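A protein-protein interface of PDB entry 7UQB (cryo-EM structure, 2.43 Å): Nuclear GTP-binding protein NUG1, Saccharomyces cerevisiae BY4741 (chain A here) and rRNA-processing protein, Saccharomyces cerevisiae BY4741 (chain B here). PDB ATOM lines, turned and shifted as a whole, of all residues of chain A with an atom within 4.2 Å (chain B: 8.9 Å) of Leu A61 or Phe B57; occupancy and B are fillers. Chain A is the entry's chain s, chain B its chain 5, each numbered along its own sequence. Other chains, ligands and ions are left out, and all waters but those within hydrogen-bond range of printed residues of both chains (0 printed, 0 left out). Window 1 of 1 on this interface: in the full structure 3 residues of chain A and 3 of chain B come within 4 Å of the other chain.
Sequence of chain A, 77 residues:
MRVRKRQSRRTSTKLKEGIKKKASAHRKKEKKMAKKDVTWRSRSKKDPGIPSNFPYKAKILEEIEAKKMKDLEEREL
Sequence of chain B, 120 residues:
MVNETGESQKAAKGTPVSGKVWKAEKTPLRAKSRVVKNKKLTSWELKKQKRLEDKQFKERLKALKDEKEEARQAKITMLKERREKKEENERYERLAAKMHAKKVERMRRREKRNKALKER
Printed residues of chain A that touch a printed residue of chain B: Lys A57, Leu A61 and Glu A65. Hydrophobic or aromatic side chains of chain A within 4 Å of the printed part of chain B: Leu A61. Of the 16 printed residues of chain B, 3 touch a printed residue of chain A. Hydrophobic or aromatic side chains of chain B within 4 Å of the printed part of chain A: Phe B57 and Leu B64. Among the printed residues, Asp or Glu carboxylates within 4 Å of a Lys or Arg side-chain nitrogen of the other chain: Lys A57 with Asp B54 (3.0 Å).
The side-chain carboxylate (OD1) of Asp B54 is in salt-bridge range of the side-chain amino group (NZ) of Lys A57 (3.0 Å).
O of Lys A57 touches CE1 of Phe B57 (3.4 Å). Phe B57 touches Leu A61 (CE1 to CD2, 3.6 Å). CD1 of Leu B64 touches CD1 of Leu A61, at 3.9 Å. Glu A65 touches Leu B64 (OE2 to CD1, 3.3 Å).
Leu A61 touches just these residues of chain B: Phe B57 and Leu B64. Of the printed residues of chain A, Phe B57 touches Lys A57 (3.4 Å) and Leu A61 (3.6 Å). Of the printed residues of chain A, Asp B54 touches Lys A57 (3.0 Å). Of the printed residues of chain B, Glu A65 touches Leu B64 (3.3 Å). Glu B53 touches none of the printed residues of chain A. The nearest printed residue of chain A that does not touch Phe B57 is Ala A58 (4.01 Å).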
ATOM      1  N   LYS A  57     -26.269  -3.022 -26.062  1.00  0.00           N
ATOM      2  CA  LYS A  57     -26.715  -4.326 -25.580  1.00  0.00           C
ATOM      3  C   LYS A  57     -25.559  -5.113 -24.985  1.00  0.00           C
ATOM      4  O   LYS A  57     -25.711  -5.759 -23.940  1.00  0.00           O
ATOM      5  CB  LYS A  57     -27.351  -5.125 -26.716  1.00  0.00           C
ATOM      6  CG  LYS A  57     -28.756  -4.724 -27.082  1.00  0.00           C
ATOM      7  CD  LYS A  57     -29.320  -5.652 -28.147  1.00  0.00           C
ATOM      8  CE  LYS A  57     -28.359  -5.810 -29.315  1.00  0.00           C
ATOM      9  NZ  LYS A  57     -28.891  -6.736 -30.350  1.00  0.00           N
ATOM     10  N   ALA A  58     -24.401  -5.085 -25.649  1.00  0.00           N
ATOM     11  CA  ALA A  58     -23.236  -5.800 -25.146  1.00  0.00           C
ATOM     12  C   ALA A  58     -22.795  -5.249 -23.799  1.00  0.00           C
ATOM     13  O   ALA A  58     -22.445  -6.014 -22.895  1.00  0.00           O
ATOM     14  CB  ALA A  58     -22.096  -5.723 -26.160  1.00  0.00           C
ATOM     15  N   LYS A  59     -22.823  -3.923 -23.642  1.00  0.00           N
ATOM     16  CA  LYS A  59     -22.462  -3.320 -22.363  1.00  0.00           C
ATOM     17  C   LYS A  59     -23.439  -3.715 -21.263  1.00  0.00           C
ATOM     18  O   LYS A  59     -23.020  -4.050 -20.149  1.00  0.00           O
ATOM     19  CB  LYS A  59     -22.394  -1.799 -22.498  1.00  0.00           C
ATOM     20  CG  LYS A  59     -21.263  -1.304 -23.381  1.00  0.00           C
ATOM     21  CD  LYS A  59     -21.157   0.212 -23.353  1.00  0.00           C
ATOM     22  CE  LYS A  59     -19.951   0.697 -24.142  1.00  0.00           C
ATOM     23  NZ  LYS A  59     -20.043   0.336 -25.585  1.00  0.00           N
ATOM     24  N   ILE A  60     -24.744  -3.692 -21.554  1.00  0.00           N
ATOM     25  CA  ILE A  60     -25.730  -4.072 -20.542  1.00  0.00           C
ATOM     26  C   ILE A  60     -25.559  -5.535 -20.145  1.00  0.00           C
ATOM     27  O   ILE A  60     -25.623  -5.885 -18.958  1.00  0.00           O
ATOM     28  CB  ILE A  60     -27.158  -3.779 -21.042  1.00  0.00           C
ATOM     29  CG1 ILE A  60     -27.355  -2.277 -21.245  1.00  0.00           C
ATOM     30  CG2 ILE A  60     -28.192  -4.300 -20.057  1.00  0.00           C
ATOM     31  CD1 ILE A  60     -27.095  -1.455 -20.005  1.00  0.00           C
ATOM     32  N   LEU A  61     -25.329  -6.408 -21.130  1.00  0.00           N
ATOM     33  CA  LEU A  61     -25.136  -7.826 -20.840  1.00  0.00           C
ATOM     34  C   LEU A  61     -23.868  -8.062 -20.025  1.00  0.00           C
ATOM     35  O   LEU A  61     -23.869  -8.869 -19.088  1.00  0.00           O
ATOM     36  CB  LEU A  61     -25.096  -8.626 -22.141  1.00  0.00           C
ATOM     37  CG  LEU A  61     -25.221 -10.140 -21.988  1.00  0.00           C
ATOM     38  CD1 LEU A  61     -26.502 -10.483 -21.250  1.00  0.00           C
ATOM     39  CD2 LEU A  61     -25.180 -10.826 -23.344  1.00  0.00           C
ATOM     40  N   GLU A  62     -22.778  -7.367 -20.365  1.00  0.00           N
ATOM     41  CA  GLU A  62     -21.546  -7.500 -19.594  1.00  0.00           C
ATOM     42  C   GLU A  62     -21.740  -7.025 -18.161  1.00  0.00           C
ATOM     43  O   GLU A  62     -21.246  -7.658 -17.221  1.00  0.00           O
ATOM     44  CB  GLU A  62     -20.416  -6.718 -20.262  1.00  0.00           C
ATOM     45  CG  GLU A  62     -19.848  -7.367 -21.512  1.00  0.00           C
ATOM     46  CD  GLU A  62     -18.898  -6.447 -22.255  1.00  0.00           C
ATOM     47  OE1 GLU A  62     -18.756  -5.280 -21.835  1.00  0.00           O
ATOM     48  OE2 GLU A  62     -18.296  -6.887 -23.257  1.00  0.00           O
ATOM     49  N   GLU A  63     -22.462  -5.917 -17.975  1.00  0.00           N
ATOM     50  CA  GLU A  63     -22.707  -5.415 -16.627  1.00  0.00           C
ATOM     51  C   GLU A  63     -23.544  -6.393 -15.811  1.00  0.00           C
ATOM     52  O   GLU A  63     -23.241  -6.646 -14.638  1.00  0.00           O
ATOM     53  CB  GLU A  63     -23.389  -4.049 -16.688  1.00  0.00           C
ATOM     54  CG  GLU A  63     -22.496  -2.931 -17.204  1.00  0.00           C
ATOM     55  CD  GLU A  63     -23.259  -1.643 -17.446  1.00  0.00           C
ATOM     56  OE1 GLU A  63     -24.300  -1.434 -16.789  1.00  0.00           O
ATOM     57  OE2 GLU A  63     -22.822  -0.842 -18.299  1.00  0.00           O
ATOM     58  N   ILE A  64     -24.596  -6.958 -16.410  1.00  0.00           N
ATOM     59  CA  ILE A  64     -25.448  -7.867 -15.647  1.00  0.00           C
ATOM     60  C   ILE A  64     -24.705  -9.166 -15.332  1.00  0.00           C
ATOM     61  O   ILE A  64     -24.842  -9.717 -14.232  1.00  0.00           O
ATOM     62  CB  ILE A  64     -26.797  -8.100 -16.363  1.00  0.00           C
ATOM     63  CG1 ILE A  64     -27.823  -8.682 -15.388  1.00  0.00           C
ATOM     64  CG2 ILE A  64     -26.671  -8.995 -17.587  1.00  0.00           C
ATOM     65  CD1 ILE A  64     -28.137  -7.771 -14.220  1.00  0.00           C
ATOM     66  N   GLU A  65     -23.868  -9.649 -16.262  1.00  0.00           N
ATOM     67  CA  GLU A  65     -23.055 -10.831 -15.981  1.00  0.00           C
ATOM     68  C   GLU A  65     -22.038 -10.563 -14.879  1.00  0.00           C
ATOM     69  O   GLU A  65     -21.824 -11.413 -14.005  1.00  0.00           O
ATOM     70  CB  GLU A  65     -22.337 -11.299 -17.245  1.00  0.00           C
ATOM     71  CG  GLU A  65     -23.224 -11.934 -18.292  1.00  0.00           C
ATOM     72  CD  GLU A  65     -22.420 -12.599 -19.389  1.00  0.00           C
ATOM     73  OE1 GLU A  65     -21.479 -13.350 -19.059  1.00  0.00           O
ATOM     74  OE2 GLU A  65     -22.720 -12.364 -20.579  1.00  0.00           O
ATOM     75  N   LYS B  50     -21.252  -4.569 -37.754  1.00  0.00           N
ATOM     76  CA  LYS B  50     -22.427  -4.546 -36.887  1.00  0.00           C
ATOM     77  C   LYS B  50     -23.175  -5.872 -36.942  1.00  0.00           C
ATOM     78  O   LYS B  50     -23.679  -6.351 -35.918  1.00  0.00           O
ATOM     79  CB  LYS B  50     -23.357  -3.395 -37.275  1.00  0.00           C
ATOM     80  CG  LYS B  50     -22.752  -2.004 -37.133  1.00  0.00           C
ATOM     81  CD  LYS B  50     -22.192  -1.760 -35.743  1.00  0.00           C
ATOM     82  CE  LYS B  50     -21.579  -0.370 -35.636  1.00  0.00           C
ATOM     83  NZ  LYS B  50     -20.446  -0.183 -36.584  1.00  0.00           N
ATOM     84  N   ARG B  51     -23.263  -6.473 -38.133  1.00  0.00           N
ATOM     85  CA  ARG B  51     -23.863  -7.798 -38.272  1.00  0.00           C
ATOM     86  C   ARG B  51     -23.140  -8.825 -37.406  1.00  0.00           C
ATOM     87  O   ARG B  51     -23.771  -9.610 -36.685  1.00  0.00           O
ATOM     88  CB  ARG B  51     -23.828  -8.226 -39.740  1.00  0.00           C
ATOM     89  CG  ARG B  51     -25.182  -8.405 -40.393  1.00  0.00           C
ATOM     90  CD  ARG B  51     -25.090  -9.359 -41.577  1.00  0.00           C
ATOM     91  NE  ARG B  51     -24.537  -8.741 -42.776  1.00  0.00           N
ATOM     92  CZ  ARG B  51     -24.289  -9.394 -43.904  1.00  0.00           C
ATOM     93  NH1 ARG B  51     -24.505 -10.694 -44.011  1.00  0.00           N
ATOM     94  NH2 ARG B  51     -23.811  -8.726 -44.949  1.00  0.00           N
ATOM     95  N   LEU B  52     -21.804  -8.827 -37.470  1.00  0.00           N
ATOM     96  CA  LEU B  52     -21.015  -9.771 -36.680  1.00  0.00           C
ATOM     97  C   LEU B  52     -21.208  -9.550 -35.184  1.00  0.00           C
ATOM     98  O   LEU B  52     -21.363 -10.513 -34.419  1.00  0.00           O
ATOM     99  CB  LEU B  52     -19.538  -9.649 -37.056  1.00  0.00           C
ATOM    100  CG  LEU B  52     -18.502 -10.281 -36.124  1.00  0.00           C
ATOM    101  CD1 LEU B  52     -18.651 -11.796 -36.067  1.00  0.00           C
ATOM    102  CD2 LEU B  52     -17.096  -9.890 -36.556  1.00  0.00           C
ATOM    103  N   GLU B  53     -21.201  -8.286 -34.750  1.00  0.00           N
ATOM    104  CA  GLU B  53     -21.390  -7.988 -33.333  1.00  0.00           C
ATOM    105  C   GLU B  53     -22.766  -8.429 -32.851  1.00  0.00           C
ATOM    106  O   GLU B  53     -22.899  -8.977 -31.748  1.00  0.00           O
ATOM    107  CB  GLU B  53     -21.192  -6.496 -33.077  1.00  0.00           C
ATOM    108  CG  GLU B  53     -19.775  -6.008 -33.303  1.00  0.00           C
ATOM    109  CD  GLU B  53     -19.683  -4.500 -33.287  1.00  0.00           C
ATOM    110  OE1 GLU B  53     -20.599  -3.857 -32.735  1.00  0.00           O
ATOM    111  OE2 GLU B  53     -18.703  -3.956 -33.836  1.00  0.00           O
ATOM    112  N   ASP B  54     -23.802  -8.198 -33.664  1.00  0.00           N
ATOM    113  CA  ASP B  54     -25.147  -8.622 -33.286  1.00  0.00           C
ATOM    114  C   ASP B  54     -25.242 -10.138 -33.191  1.00  0.00           C
ATOM    115  O   ASP B  54     -25.872 -10.667 -32.267  1.00  0.00           O
ATOM    116  CB  ASP B  54     -26.172  -8.081 -34.281  1.00  0.00           C
ATOM    117  CG  ASP B  54     -27.589  -8.498 -33.938  1.00  0.00           C
ATOM    118  OD1 ASP B  54     -28.143  -7.971 -32.950  1.00  0.00           O
ATOM    119  OD2 ASP B  54     -28.146  -9.355 -34.653  1.00  0.00           O
ATOM    120  N   LYS B  55     -24.620 -10.857 -34.132  1.00  0.00           N
ATOM    121  CA  LYS B  55     -24.637 -12.316 -34.074  1.00  0.00           C
ATOM    122  C   LYS B  55     -23.938 -12.833 -32.819  1.00  0.00           C
ATOM    123  O   LYS B  55     -24.429 -13.759 -32.159  1.00  0.00           O
ATOM    124  CB  LYS B  55     -23.986 -12.902 -35.327  1.00  0.00           C
ATOM    125  CG  LYS B  55     -24.818 -12.764 -36.592  1.00  0.00           C
ATOM    126  CD  LYS B  55     -24.050 -13.262 -37.806  1.00  0.00           C
ATOM    127  CE  LYS B  55     -24.913 -13.251 -39.059  1.00  0.00           C
ATOM    128  NZ  LYS B  55     -25.381 -11.881 -39.403  1.00  0.00           N
ATOM    129  N   GLN B  56     -22.790 -12.240 -32.474  1.00  0.00           N
ATOM    130  CA  GLN B  56     -22.068 -12.673 -31.279  1.00  0.00           C
ATOM    131  C   GLN B  56     -22.860 -12.381 -30.007  1.00  0.00           C
ATOM    132  O   GLN B  56     -22.914 -13.220 -29.095  1.00  0.00           O
ATOM    133  CB  GLN B  56     -20.691 -12.015 -31.239  1.00  0.00           C
ATOM    134  CG  GLN B  56     -19.754 -12.539 -32.316  1.00  0.00           C
ATOM    135  CD  GLN B  56     -18.443 -11.784 -32.384  1.00  0.00           C
ATOM    136  OE1 GLN B  56     -18.358 -10.622 -31.985  1.00  0.00           O
ATOM    137  NE2 GLN B  56     -17.409 -12.444 -32.891  1.00  0.00           N
ATOM    138  N   PHE B  57     -23.497 -11.207 -29.932  1.00  0.00           N
ATOM    139  CA  PHE B  57     -24.346 -10.901 -28.784  1.00  0.00           C
ATOM    140  C   PHE B  57     -25.502 -11.887 -28.677  1.00  0.00           C
ATOM    141  O   PHE B  57     -25.836 -12.349 -27.578  1.00  0.00           O
ATOM    142  CB  PHE B  57     -24.873  -9.466 -28.879  1.00  0.00           C
ATOM    143  CG  PHE B  57     -25.968  -9.153 -27.891  1.00  0.00           C
ATOM    144  CD1 PHE B  57     -25.664  -8.772 -26.597  1.00  0.00           C
ATOM    145  CD2 PHE B  57     -27.305  -9.236 -28.261  1.00  0.00           C
ATOM    146  CE1 PHE B  57     -26.666  -8.486 -25.689  1.00  0.00           C
ATOM    147  CE2 PHE B  57     -28.308  -8.958 -27.356  1.00  0.00           C
ATOM    148  CZ  PHE B  57     -27.988  -8.579 -26.069  1.00  0.00           C
ATOM    149  N   LYS B  58     -26.131 -12.210 -29.810  1.00  0.00           N
ATOM    150  CA  LYS B  58     -27.276 -13.114 -29.789  1.00  0.00           C
ATOM    151  C   LYS B  58     -26.875 -14.508 -29.330  1.00  0.00           C
ATOM    152  O   LYS B  58     -27.587 -15.130 -28.533  1.00  0.00           O
ATOM    153  CB  LYS B  58     -27.934 -13.168 -31.167  1.00  0.00           C
ATOM    154  CG  LYS B  58     -28.725 -11.918 -31.519  1.00  0.00           C
ATOM    155  CD  LYS B  58     -29.417 -12.060 -32.863  1.00  0.00           C
ATOM    156  CE  LYS B  58     -30.402 -13.214 -32.851  1.00  0.00           C
ATOM    157  NZ  LYS B  58     -31.419 -13.064 -31.772  1.00  0.00           N
ATOM    158  N   GLU B  59     -25.733 -15.017 -29.805  1.00  0.00           N
ATOM    159  CA  GLU B  59     -25.327 -16.353 -29.371  1.00  0.00           C
ATOM    160  C   GLU B  59     -24.895 -16.365 -27.904  1.00  0.00           C
ATOM    161  O   GLU B  59     -25.159 -17.347 -27.196  1.00  0.00           O
ATOM    162  CB  GLU B  59     -24.228 -16.913 -30.278  1.00  0.00           C
ATOM    163  CG  GLU B  59     -22.952 -16.106 -30.348  1.00  0.00           C
ATOM    164  CD  GLU B  59     -21.930 -16.712 -31.289  1.00  0.00           C
ATOM    165  OE1 GLU B  59     -22.017 -17.928 -31.558  1.00  0.00           O
ATOM    166  OE2 GLU B  59     -21.041 -15.972 -31.763  1.00  0.00           O
ATOM    167  N   ARG B  60     -24.270 -15.285 -27.419  1.00  0.00           N
ATOM    168  CA  ARG B  60     -23.935 -15.201 -25.998  1.00  0.00           C
ATOM    169  C   ARG B  60     -25.195 -15.212 -25.131  1.00  0.00           C
ATOM    170  O   ARG B  60     -25.280 -15.948 -24.134  1.00  0.00           O
ATOM    171  CB  ARG B  60     -23.111 -13.938 -25.739  1.00  0.00           C
ATOM    172  CG  ARG B  60     -22.523 -13.825 -24.342  1.00  0.00           C
ATOM    173  CD  ARG B  60     -21.101 -14.369 -24.286  1.00  0.00           C
ATOM    174  NE  ARG B  60     -21.061 -15.826 -24.302  1.00  0.00           N
ATOM    175  CZ  ARG B  60     -19.944 -16.542 -24.350  1.00  0.00           C
ATOM    176  NH1 ARG B  60     -18.756 -15.967 -24.413  1.00  0.00           N
ATOM    177  NH2 ARG B  60     -20.024 -17.870 -24.336  1.00  0.00           N
ATOM    178  N   LEU B  61     -26.195 -14.412 -25.514  1.00  0.00           N
ATOM    179  CA  LEU B  61     -27.448 -14.374 -24.764  1.00  0.00           C
ATOM    180  C   LEU B  61     -28.175 -15.711 -24.830  1.00  0.00           C
ATOM    181  O   LEU B  61     -28.787 -16.144 -23.846  1.00  0.00           O
ATOM    182  CB  LEU B  61     -28.340 -13.251 -25.293  1.00  0.00           C
ATOM    183  CG  LEU B  61     -29.677 -13.066 -24.573  1.00  0.00           C
ATOM    184  CD1 LEU B  61     -29.455 -12.635 -23.130  1.00  0.00           C
ATOM    185  CD2 LEU B  61     -30.561 -12.073 -25.309  1.00  0.00           C
ATOM    186  N   LYS B  62     -28.124 -16.376 -25.989  1.00  0.00           N
ATOM    187  CA  LYS B  62     -28.744 -17.689 -26.129  1.00  0.00           C
ATOM    188  C   LYS B  62     -28.089 -18.707 -25.207  1.00  0.00           C
ATOM    189  O   LYS B  62     -28.778 -19.523 -24.585  1.00  0.00           O
ATOM    190  CB  LYS B  62     -28.666 -18.146 -27.585  1.00  0.00           C
ATOM    191  CG  LYS B  62     -29.347 -19.477 -27.878  1.00  0.00           C
ATOM    192  CD  LYS B  62     -29.231 -19.830 -29.357  1.00  0.00           C
ATOM    193  CE  LYS B  62     -29.977 -21.113 -29.698  1.00  0.00           C
ATOM    194  NZ  LYS B  62     -29.387 -22.306 -29.029  1.00  0.00           N
ATOM    195  N   ALA B  63     -26.756 -18.669 -25.102  1.00  0.00           N
ATOM    196  CA  ALA B  63     -26.062 -19.570 -24.186  1.00  0.00           C
ATOM    197  C   ALA B  63     -26.463 -19.309 -22.738  1.00  0.00           C
ATOM    198  O   ALA B  63     -26.695 -20.254 -21.968  1.00  0.00           O
ATOM    199  CB  ALA B  63     -24.551 -19.430 -24.357  1.00  0.00           C
ATOM    200  N   LEU B  64     -26.553 -18.031 -22.349  1.00  0.00           N
ATOM    201  CA  LEU B  64     -26.947 -17.706 -20.977  1.00  0.00           C
ATOM    202  C   LEU B  64     -28.368 -18.179 -20.674  1.00  0.00           C
ATOM    203  O   LEU B  64     -28.627 -18.764 -19.610  1.00  0.00           O
ATOM    204  CB  LEU B  64     -26.824 -16.205 -20.735  1.00  0.00           C
ATOM    205  CG  LEU B  64     -25.419 -15.618 -20.863  1.00  0.00           C
ATOM    206  CD1 LEU B  64     -25.423 -14.165 -20.427  1.00  0.00           C
ATOM    207  CD2 LEU B  64     -24.422 -16.429 -20.052  1.00  0.00           C
ATOM    208  N   LYS B  65     -29.299 -17.944 -21.600  1.00  0.00           N
ATOM    209  CA  LYS B  65     -30.675 -18.388 -21.394  1.00  0.00           C
ATOM    210  C   LYS B  65     -30.765 -19.908 -21.342  1.00  0.00           C
ATOM    211  O   LYS B  65     -31.522 -20.465 -20.535  1.00  0.00           O
ATOM    212  CB  LYS B  65     -31.574 -17.829 -22.494  1.00  0.00           C
ATOM    213  CG  LYS B  65     -31.767 -16.323 -22.418  1.00  0.00           C
ATOM    214  CD  LYS B  65     -32.514 -15.794 -23.627  1.00  0.00           C
ATOM    215  CE  LYS B  65     -32.951 -14.354 -23.417  1.00  0.00           C
ATOM    216  NZ  LYS B  65     -33.958 -14.241 -22.325  1.00  0.00           N
